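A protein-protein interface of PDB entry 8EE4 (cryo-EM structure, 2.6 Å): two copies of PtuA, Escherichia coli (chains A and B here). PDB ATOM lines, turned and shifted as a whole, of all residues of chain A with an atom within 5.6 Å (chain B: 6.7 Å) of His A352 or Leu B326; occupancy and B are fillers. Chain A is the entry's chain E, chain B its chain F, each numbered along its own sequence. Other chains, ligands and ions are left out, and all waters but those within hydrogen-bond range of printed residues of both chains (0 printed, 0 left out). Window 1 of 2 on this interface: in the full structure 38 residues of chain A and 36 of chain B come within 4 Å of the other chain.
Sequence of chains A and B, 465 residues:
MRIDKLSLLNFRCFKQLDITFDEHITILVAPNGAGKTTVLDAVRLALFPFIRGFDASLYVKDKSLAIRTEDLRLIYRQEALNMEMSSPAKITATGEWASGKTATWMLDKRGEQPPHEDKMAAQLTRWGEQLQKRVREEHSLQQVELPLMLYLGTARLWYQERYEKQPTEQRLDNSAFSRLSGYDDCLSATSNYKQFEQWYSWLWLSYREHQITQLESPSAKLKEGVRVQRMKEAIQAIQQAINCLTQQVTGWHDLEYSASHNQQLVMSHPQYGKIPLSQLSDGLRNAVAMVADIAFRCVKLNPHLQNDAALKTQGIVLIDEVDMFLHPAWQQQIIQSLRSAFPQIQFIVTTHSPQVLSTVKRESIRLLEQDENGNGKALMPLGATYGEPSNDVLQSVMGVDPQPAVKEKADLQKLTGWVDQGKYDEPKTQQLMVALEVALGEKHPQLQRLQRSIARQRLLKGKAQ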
ATOM      1  N   VAL A  29      17.846  -0.249  20.518  1.00  0.00           N
ATOM      2  CA  VAL A  29      16.880  -0.514  21.578  1.00  0.00           C
ATOM      3  C   VAL A  29      17.233   0.357  22.776  1.00  0.00           C
ATOM      4  O   VAL A  29      18.394   0.402  23.195  1.00  0.00           O
ATOM      5  CB  VAL A  29      16.864  -2.003  21.976  1.00  0.00           C
ATOM      6  CG1 VAL A  29      15.968  -2.226  23.182  1.00  0.00           C
ATOM      7  CG2 VAL A  29      16.413  -2.858  20.805  1.00  0.00           C
ATOM      8  N   LYS A  36      17.311   7.057  20.956  1.00  0.00           N
ATOM      9  CA  LYS A  36      17.232   6.463  19.627  1.00  0.00           C
ATOM     10  C   LYS A  36      17.001   7.537  18.572  1.00  0.00           C
ATOM     11  O   LYS A  36      17.666   7.559  17.527  1.00  0.00           O
ATOM     12  CB  LYS A  36      16.115   5.420  19.587  1.00  0.00           C
ATOM     13  CG  LYS A  36      16.285   4.291  20.588  1.00  0.00           C
ATOM     14  CD  LYS A  36      15.356   3.125  20.284  1.00  0.00           C
ATOM     15  CE  LYS A  36      13.894   3.537  20.356  1.00  0.00           C
ATOM     16  NZ  LYS A  36      12.995   2.370  20.573  1.00  0.00           N
ATOM     17  N   GLU A 321      10.653   3.303  14.399  1.00  0.00           N
ATOM     18  CA  GLU A 321       9.450   2.512  14.655  1.00  0.00           C
ATOM     19  C   GLU A 321       9.035   1.743  13.396  1.00  0.00           C
ATOM     20  O   GLU A 321       7.985   1.978  12.796  1.00  0.00           O
ATOM     21  CB  GLU A 321       8.310   3.408  15.155  1.00  0.00           C
ATOM     22  CG  GLU A 321       8.719   4.418  16.217  1.00  0.00           C
ATOM     23  CD  GLU A 321       9.082   3.769  17.536  1.00  0.00           C
ATOM     24  OE1 GLU A 321       8.950   2.533  17.649  1.00  0.00           O
ATOM     25  OE2 GLU A 321       9.500   4.497  18.460  1.00  0.00           O
ATOM     26  N   ASP A 323       8.152  -1.377  12.925  1.00  0.00           N
ATOM     27  CA  ASP A 323       7.038  -2.313  13.038  1.00  0.00           C
ATOM     28  C   ASP A 323       5.764  -1.651  13.551  1.00  0.00           C
ATOM     29  O   ASP A 323       4.953  -2.304  14.219  1.00  0.00           O
ATOM     30  CB  ASP A 323       7.429  -3.479  13.945  1.00  0.00           C
ATOM     31  CG  ASP A 323       7.490  -3.086  15.407  1.00  0.00           C
ATOM     32  OD1 ASP A 323       8.360  -2.267  15.770  1.00  0.00           O
ATOM     33  OD2 ASP A 323       6.665  -3.597  16.193  1.00  0.00           O
ATOM     34  N   THR A 350      14.739   1.363  14.457  1.00  0.00           N
ATOM     35  CA  THR A 350      14.447   1.364  15.886  1.00  0.00           C
ATOM     36  C   THR A 350      13.162   0.591  16.169  1.00  0.00           C
ATOM     37  O   THR A 350      12.185   0.702  15.424  1.00  0.00           O
ATOM     38  CB  THR A 350      14.319   2.791  16.434  1.00  0.00           C
ATOM     39  OG1 THR A 350      13.051   3.342  16.057  1.00  0.00           O
ATOM     40  CG2 THR A 350      15.439   3.674  15.909  1.00  0.00           C
ATOM     41  N   THR A 351      13.171  -0.186  17.254  1.00  0.00           N
ATOM     42  CA  THR A 351      12.010  -0.967  17.669  1.00  0.00           C
ATOM     43  C   THR A 351      12.049  -1.171  19.178  1.00  0.00           C
ATOM     44  O   THR A 351      13.063  -0.930  19.836  1.00  0.00           O
ATOM     45  CB  THR A 351      11.953  -2.344  16.986  1.00  0.00           C
ATOM     46  OG1 THR A 351      13.017  -3.170  17.475  1.00  0.00           O
ATOM     47  CG2 THR A 351      12.065  -2.217  15.482  1.00  0.00           C
ATOM     48  N   HIS A 352      10.912  -1.620  19.723  1.00  0.00           N
ATOM     49  CA  HIS A 352      10.846  -2.111  21.096  1.00  0.00           C
ATOM     50  C   HIS A 352       9.989  -3.370  21.182  1.00  0.00           C
ATOM     51  O   HIS A 352       9.313  -3.597  22.191  1.00  0.00           O
ATOM     52  CB  HIS A 352      10.304  -1.041  22.050  1.00  0.00           C
ATOM     53  CG  HIS A 352       8.936  -0.544  21.696  1.00  0.00           C
ATOM     54  ND1 HIS A 352       8.681   0.776  21.391  1.00  0.00           N
ATOM     55  CD2 HIS A 352       7.746  -1.184  21.614  1.00  0.00           C
ATOM     56  CE1 HIS A 352       7.395   0.925  21.127  1.00  0.00           C
ATOM     57  NE2 HIS A 352       6.806  -0.249  21.254  1.00  0.00           N
ATOM     58  N   SER A 353      10.014  -4.201  20.140  1.00  0.00           N
ATOM     59  CA  SER A 353       9.146  -5.367  20.043  1.00  0.00           C
ATOM     60  C   SER A 353       9.966  -6.641  20.176  1.00  0.00           C
ATOM     61  O   SER A 353      10.884  -6.854  19.370  1.00  0.00           O
ATOM     62  CB  SER A 353       8.399  -5.360  18.712  1.00  0.00           C
ATOM     63  OG  SER A 353       7.912  -6.651  18.399  1.00  0.00           O
ATOM     64  N   PRO A 354       9.690  -7.513  21.152  1.00  0.00           N
ATOM     65  CA  PRO A 354      10.450  -8.772  21.231  1.00  0.00           C
ATOM     66  C   PRO A 354      10.309  -9.645  19.997  1.00  0.00           C
ATOM     67  O   PRO A 354      11.231 -10.408  19.683  1.00  0.00           O
ATOM     68  CB  PRO A 354       9.869  -9.460  22.475  1.00  0.00           C
ATOM     69  CG  PRO A 354       8.559  -8.792  22.717  1.00  0.00           C
ATOM     70  CD  PRO A 354       8.735  -7.384  22.264  1.00  0.00           C
ATOM     71  N   MET A 398      15.387  -7.004  27.347  1.00  0.00           N
ATOM     72  CA  MET A 398      14.631  -5.830  27.756  1.00  0.00           C
ATOM     73  C   MET A 398      14.296  -5.809  29.240  1.00  0.00           C
ATOM     74  O   MET A 398      13.803  -4.786  29.728  1.00  0.00           O
ATOM     75  CB  MET A 398      13.329  -5.735  26.945  1.00  0.00           C
ATOM     76  CG  MET A 398      13.439  -6.299  25.533  1.00  0.00           C
ATOM     77  SD  MET A 398      11.916  -6.139  24.584  1.00  0.00           S
ATOM     78  CE  MET A 398      11.806  -4.361  24.420  1.00  0.00           C
ATOM     79  N   GLY B 283       6.727   8.333  24.388  1.00  0.00           N
ATOM     80  CA  GLY B 283       5.554   7.487  24.470  1.00  0.00           C
ATOM     81  C   GLY B 283       4.780   7.671  25.758  1.00  0.00           C
ATOM     82  O   GLY B 283       3.554   7.813  25.739  1.00  0.00           O
ATOM     83  N   LEU B 284       5.489   7.671  26.890  1.00  0.00           N
ATOM     84  CA  LEU B 284       4.830   7.851  28.179  1.00  0.00           C
ATOM     85  C   LEU B 284       4.281   9.264  28.337  1.00  0.00           C
ATOM     86  O   LEU B 284       3.256   9.465  29.004  1.00  0.00           O
ATOM     87  CB  LEU B 284       5.811   7.527  29.306  1.00  0.00           C
ATOM     88  CG  LEU B 284       5.363   7.834  30.734  1.00  0.00           C
ATOM     89  CD1 LEU B 284       4.072   7.106  31.069  1.00  0.00           C
ATOM     90  CD2 LEU B 284       6.460   7.452  31.710  1.00  0.00           C
ATOM     91  N   ALA B 287       0.893   9.247  26.887  1.00  0.00           N
ATOM     92  CA  ALA B 287      -0.054   8.574  27.772  1.00  0.00           C
ATOM     93  C   ALA B 287      -0.503   9.499  28.897  1.00  0.00           C
ATOM     94  O   ALA B 287      -1.698   9.564  29.230  1.00  0.00           O
ATOM     95  CB  ALA B 287       0.578   7.305  28.342  1.00  0.00           C
ATOM     96  N   VAL B 322      -4.810   1.144  21.948  1.00  0.00           N
ATOM     97  CA  VAL B 322      -4.528   1.684  23.274  1.00  0.00           C
ATOM     98  C   VAL B 322      -3.061   1.540  23.653  1.00  0.00           C
ATOM     99  O   VAL B 322      -2.575   2.272  24.522  1.00  0.00           O
ATOM    100  CB  VAL B 322      -5.426   0.993  24.322  1.00  0.00           C
ATOM    101  CG1 VAL B 322      -4.921  -0.416  24.605  1.00  0.00           C
ATOM    102  CG2 VAL B 322      -5.487   1.820  25.603  1.00  0.00           C
ATOM    103  N   ASP B 323      -2.336   0.614  23.024  1.00  0.00           N
ATOM    104  CA  ASP B 323      -0.948   0.332  23.363  1.00  0.00           C
ATOM    105  C   ASP B 323       0.035   0.942  22.369  1.00  0.00           C
ATOM    106  O   ASP B 323       1.186   0.500  22.295  1.00  0.00           O
ATOM    107  CB  ASP B 323      -0.730  -1.179  23.444  1.00  0.00           C
ATOM    108  CG  ASP B 323      -1.058  -1.882  22.142  1.00  0.00           C
ATOM    109  OD1 ASP B 323      -1.676  -1.249  21.260  1.00  0.00           O
ATOM    110  OD2 ASP B 323      -0.693  -3.065  21.994  1.00  0.00           O
ATOM    111  N   MET B 324      -0.393   1.940  21.604  1.00  0.00           N
ATOM    112  CA  MET B 324       0.461   2.515  20.574  1.00  0.00           C
ATOM    113  C   MET B 324       1.617   3.285  21.203  1.00  0.00           C
ATOM    114  O   MET B 324       1.416   4.108  22.102  1.00  0.00           O
ATOM    115  CB  MET B 324      -0.366   3.427  19.669  1.00  0.00           C
ATOM    116  CG  MET B 324       0.438   4.250  18.683  1.00  0.00           C
ATOM    117  SD  MET B 324      -0.620   5.033  17.449  1.00  0.00           S
ATOM    118  CE  MET B 324      -1.130   6.513  18.315  1.00  0.00           C
ATOM    119  N   PHE B 325       2.833   3.015  20.721  1.00  0.00           N
ATOM    120  CA  PHE B 325       4.046   3.689  21.193  1.00  0.00           C
ATOM    121  C   PHE B 325       4.240   3.511  22.696  1.00  0.00           C
ATOM    122  O   PHE B 325       4.598   4.453  23.407  1.00  0.00           O
ATOM    123  CB  PHE B 325       4.029   5.176  20.831  1.00  0.00           C
ATOM    124  CG  PHE B 325       4.167   5.452  19.361  1.00  0.00           C
ATOM    125  CD1 PHE B 325       5.126   4.805  18.600  1.00  0.00           C
ATOM    126  CD2 PHE B 325       3.342   6.374  18.741  1.00  0.00           C
ATOM    127  CE1 PHE B 325       5.249   5.066  17.252  1.00  0.00           C
ATOM    128  CE2 PHE B 325       3.465   6.639  17.395  1.00  0.00           C
ATOM    129  CZ  PHE B 325       4.419   5.985  16.650  1.00  0.00           C
ATOM    130  N   LEU B 326       4.009   2.298  23.191  1.00  0.00           N
ATOM    131  CA  LEU B 326       4.177   1.983  24.603  1.00  0.00           C
ATOM    132  C   LEU B 326       5.149   0.824  24.756  1.00  0.00           C
ATOM    133  O   LEU B 326       5.055  -0.172  24.031  1.00  0.00           O
ATOM    134  CB  LEU B 326       2.834   1.636  25.260  1.00  0.00           C
ATOM    135  CG  LEU B 326       2.006   2.789  25.841  1.00  0.00           C
ATOM    136  CD1 LEU B 326       0.812   2.248  26.611  1.00  0.00           C
ATOM    137  CD2 LEU B 326       2.839   3.693  26.739  1.00  0.00           C
ATOM    138  N   HIS B 327       6.074   0.958  25.702  1.00  0.00           N
ATOM    139  CA  HIS B 327       7.026  -0.101  25.981  1.00  0.00           C
ATOM    140  C   HIS B 327       6.300  -1.314  26.564  1.00  0.00           C
ATOM    141  O   HIS B 327       5.263  -1.168  27.216  1.00  0.00           O
ATOM    142  CB  HIS B 327       8.089   0.394  26.958  1.00  0.00           C
ATOM    143  CG  HIS B 327       9.409  -0.296  26.824  1.00  0.00           C
ATOM    144  ND1 HIS B 327       9.828  -1.277  27.697  1.00  0.00           N
ATOM    145  CD2 HIS B 327      10.405  -0.149  25.919  1.00  0.00           C
ATOM    146  CE1 HIS B 327      11.024  -1.703  27.336  1.00  0.00           C
ATOM    147  NE2 HIS B 327      11.398  -1.035  26.260  1.00  0.00           N
ATOM    148  N   PRO B 328       6.821  -2.527  26.351  1.00  0.00           N
ATOM    149  CA  PRO B 328       6.143  -3.711  26.904  1.00  0.00           C
ATOM    150  C   PRO B 328       5.944  -3.653  28.407  1.00  0.00           C
ATOM    151  O   PRO B 328       5.084  -4.373  28.929  1.00  0.00           O
ATOM    152  CB  PRO B 328       7.074  -4.863  26.506  1.00  0.00           C
ATOM    153  CG  PRO B 328       7.753  -4.385  25.284  1.00  0.00           C
ATOM    154  CD  PRO B 328       7.931  -2.903  25.457  1.00  0.00           C
ATOM    155  N   ALA B 329       6.709  -2.827  29.122  1.00  0.00           N
ATOM    156  CA  ALA B 329       6.496  -2.678  30.557  1.00  0.00           C
ATOM    157  C   ALA B 329       5.243  -1.863  30.852  1.00  0.00           C
ATOM    158  O   ALA B 329       4.489  -2.193  31.774  1.00  0.00           O
ATOM    159  CB  ALA B 329       7.716  -2.024  31.203  1.00  0.00           C
ATOM    160  N   TRP B 330       5.003  -0.799  30.083  1.00  0.00           N
ATOM    161  CA  TRP B 330       3.823   0.030  30.288  1.00  0.00           C
ATOM    162  C   TRP B 330       2.558  -0.596  29.722  1.00  0.00           C
ATOM    163  O   TRP B 330       1.457  -0.201  30.120  1.00  0.00           O
ATOM    164  CB  TRP B 330       4.033   1.409  29.657  1.00  0.00           C
ATOM    165  CG  TRP B 330       4.973   2.281  30.426  1.00  0.00           C
ATOM    166  CD1 TRP B 330       6.236   2.646  30.061  1.00  0.00           C
ATOM    167  CD2 TRP B 330       4.728   2.899  31.694  1.00  0.00           C
ATOM    168  NE1 TRP B 330       6.792   3.452  31.025  1.00  0.00           N
ATOM    169  CE2 TRP B 330       5.885   3.624  32.037  1.00  0.00           C
ATOM    170  CE3 TRP B 330       3.640   2.910  32.573  1.00  0.00           C
ATOM    171  CZ2 TRP B 330       5.988   4.351  33.220  1.00  0.00           C
ATOM    172  CZ3 TRP B 330       3.744   3.633  33.746  1.00  0.00           C
ATOM    173  CH2 TRP B 330       4.909   4.344  34.059  1.00  0.00           C
ATOM    174  N   GLN B 331       2.684  -1.558  28.808  1.00  0.00           N
ATOM    175  CA  GLN B 331       1.510  -2.205  28.239  1.00  0.00           C
ATOM    176  C   GLN B 331       0.797  -3.099  29.244  1.00  0.00           C
ATOM    177  O   GLN B 331      -0.335  -3.519  28.986  1.00  0.00           O
ATOM    178  CB  GLN B 331       1.907  -3.021  27.008  1.00  0.00           C
ATOM    179  CG  GLN B 331       2.411  -2.178  25.847  1.00  0.00           C
ATOM    180  CD  GLN B 331       2.891  -3.019  24.681  1.00  0.00           C
ATOM    181  OE1 GLN B 331       2.784  -4.244  24.699  1.00  0.00           O
ATOM    182  NE2 GLN B 331       3.427  -2.363  23.659  1.00  0.00           N
ATOM    183  N   ILE B 334      -1.731  -0.243  31.584  1.00  0.00           N
ATOM    184  CA  ILE B 334      -2.556   0.829  31.032  1.00  0.00           C
ATOM    185  C   ILE B 334      -4.032   0.580  31.322  1.00  0.00           C
ATOM    186  O   ILE B 334      -4.765   1.497  31.717  1.00  0.00           O
ATOM    187  CB  ILE B 334      -2.285   0.982  29.522  1.00  0.00           C
ATOM    188  CG1 ILE B 334      -2.990   2.223  28.969  1.00  0.00           C
ATOM    189  CG2 ILE B 334      -2.734  -0.254  28.759  1.00  0.00           C
ATOM    190  CD1 ILE B 334      -2.327   3.522  29.352  1.00  0.00           C
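The backbone carbonyl oxygen of Leu B326 is in hydrogen-bond range of a ring nitrogen (NE2) of His A352, 3.3 Å away.
The side-chain amide nitrogen of Gln B331 is in hydrogen-bond range of the backbone carbonyl oxygen of Leu B326, at 2.8 Å. N of Glu A321 is in hydrogen-bond range of OG1 of Thr A350.
Among the printed residues, pairs that only touch across the chains: His A352 with Pro B328 (3.6 Å), Glu A321 with Phe B325 (3.7 Å), Met A398 with His B327 (3.8 Å) and His A352 with His B327 (3.97 Å).
Printed residues of chain B within 4 Å of Glu A321: Phe B325. His A352 touches just these residues of chain B: Leu B326 (3.3 Å), His B327 (3.97 Å) and Pro B328 (3.6 Å). Of the printed residues of chain B, Met A398 touches His B327 (3.8 Å). Printed residues of chain A within 4 Å of Phe B325: Glu A321. Printed residues of chain A within 4 Å of His B327: His A352 and Met A398. Printed residues of chain A within 4 Å of Pro B328: His A352. Ile B334 touches none of the printed residues of chain A. The nearest printed residue of chain A that does not touch Leu B326 is Glu A321 (7.4 Å).
Of the 14 printed residues of chain B, 4 touch a printed residue of chain A. Hydrophobic or aromatic side chains of chain B within 4 Å of the printed part of chain A: Phe B325, His B327 and Pro B328. Hydrophobic or aromatic side chains of chain A that line the printed part of chain B: His A352 and Met A398.
Position printed for both chains: 323. Of the 5 pairs that touch across the chains among the printed residues, none has its exchanged pair printed and touching as well.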
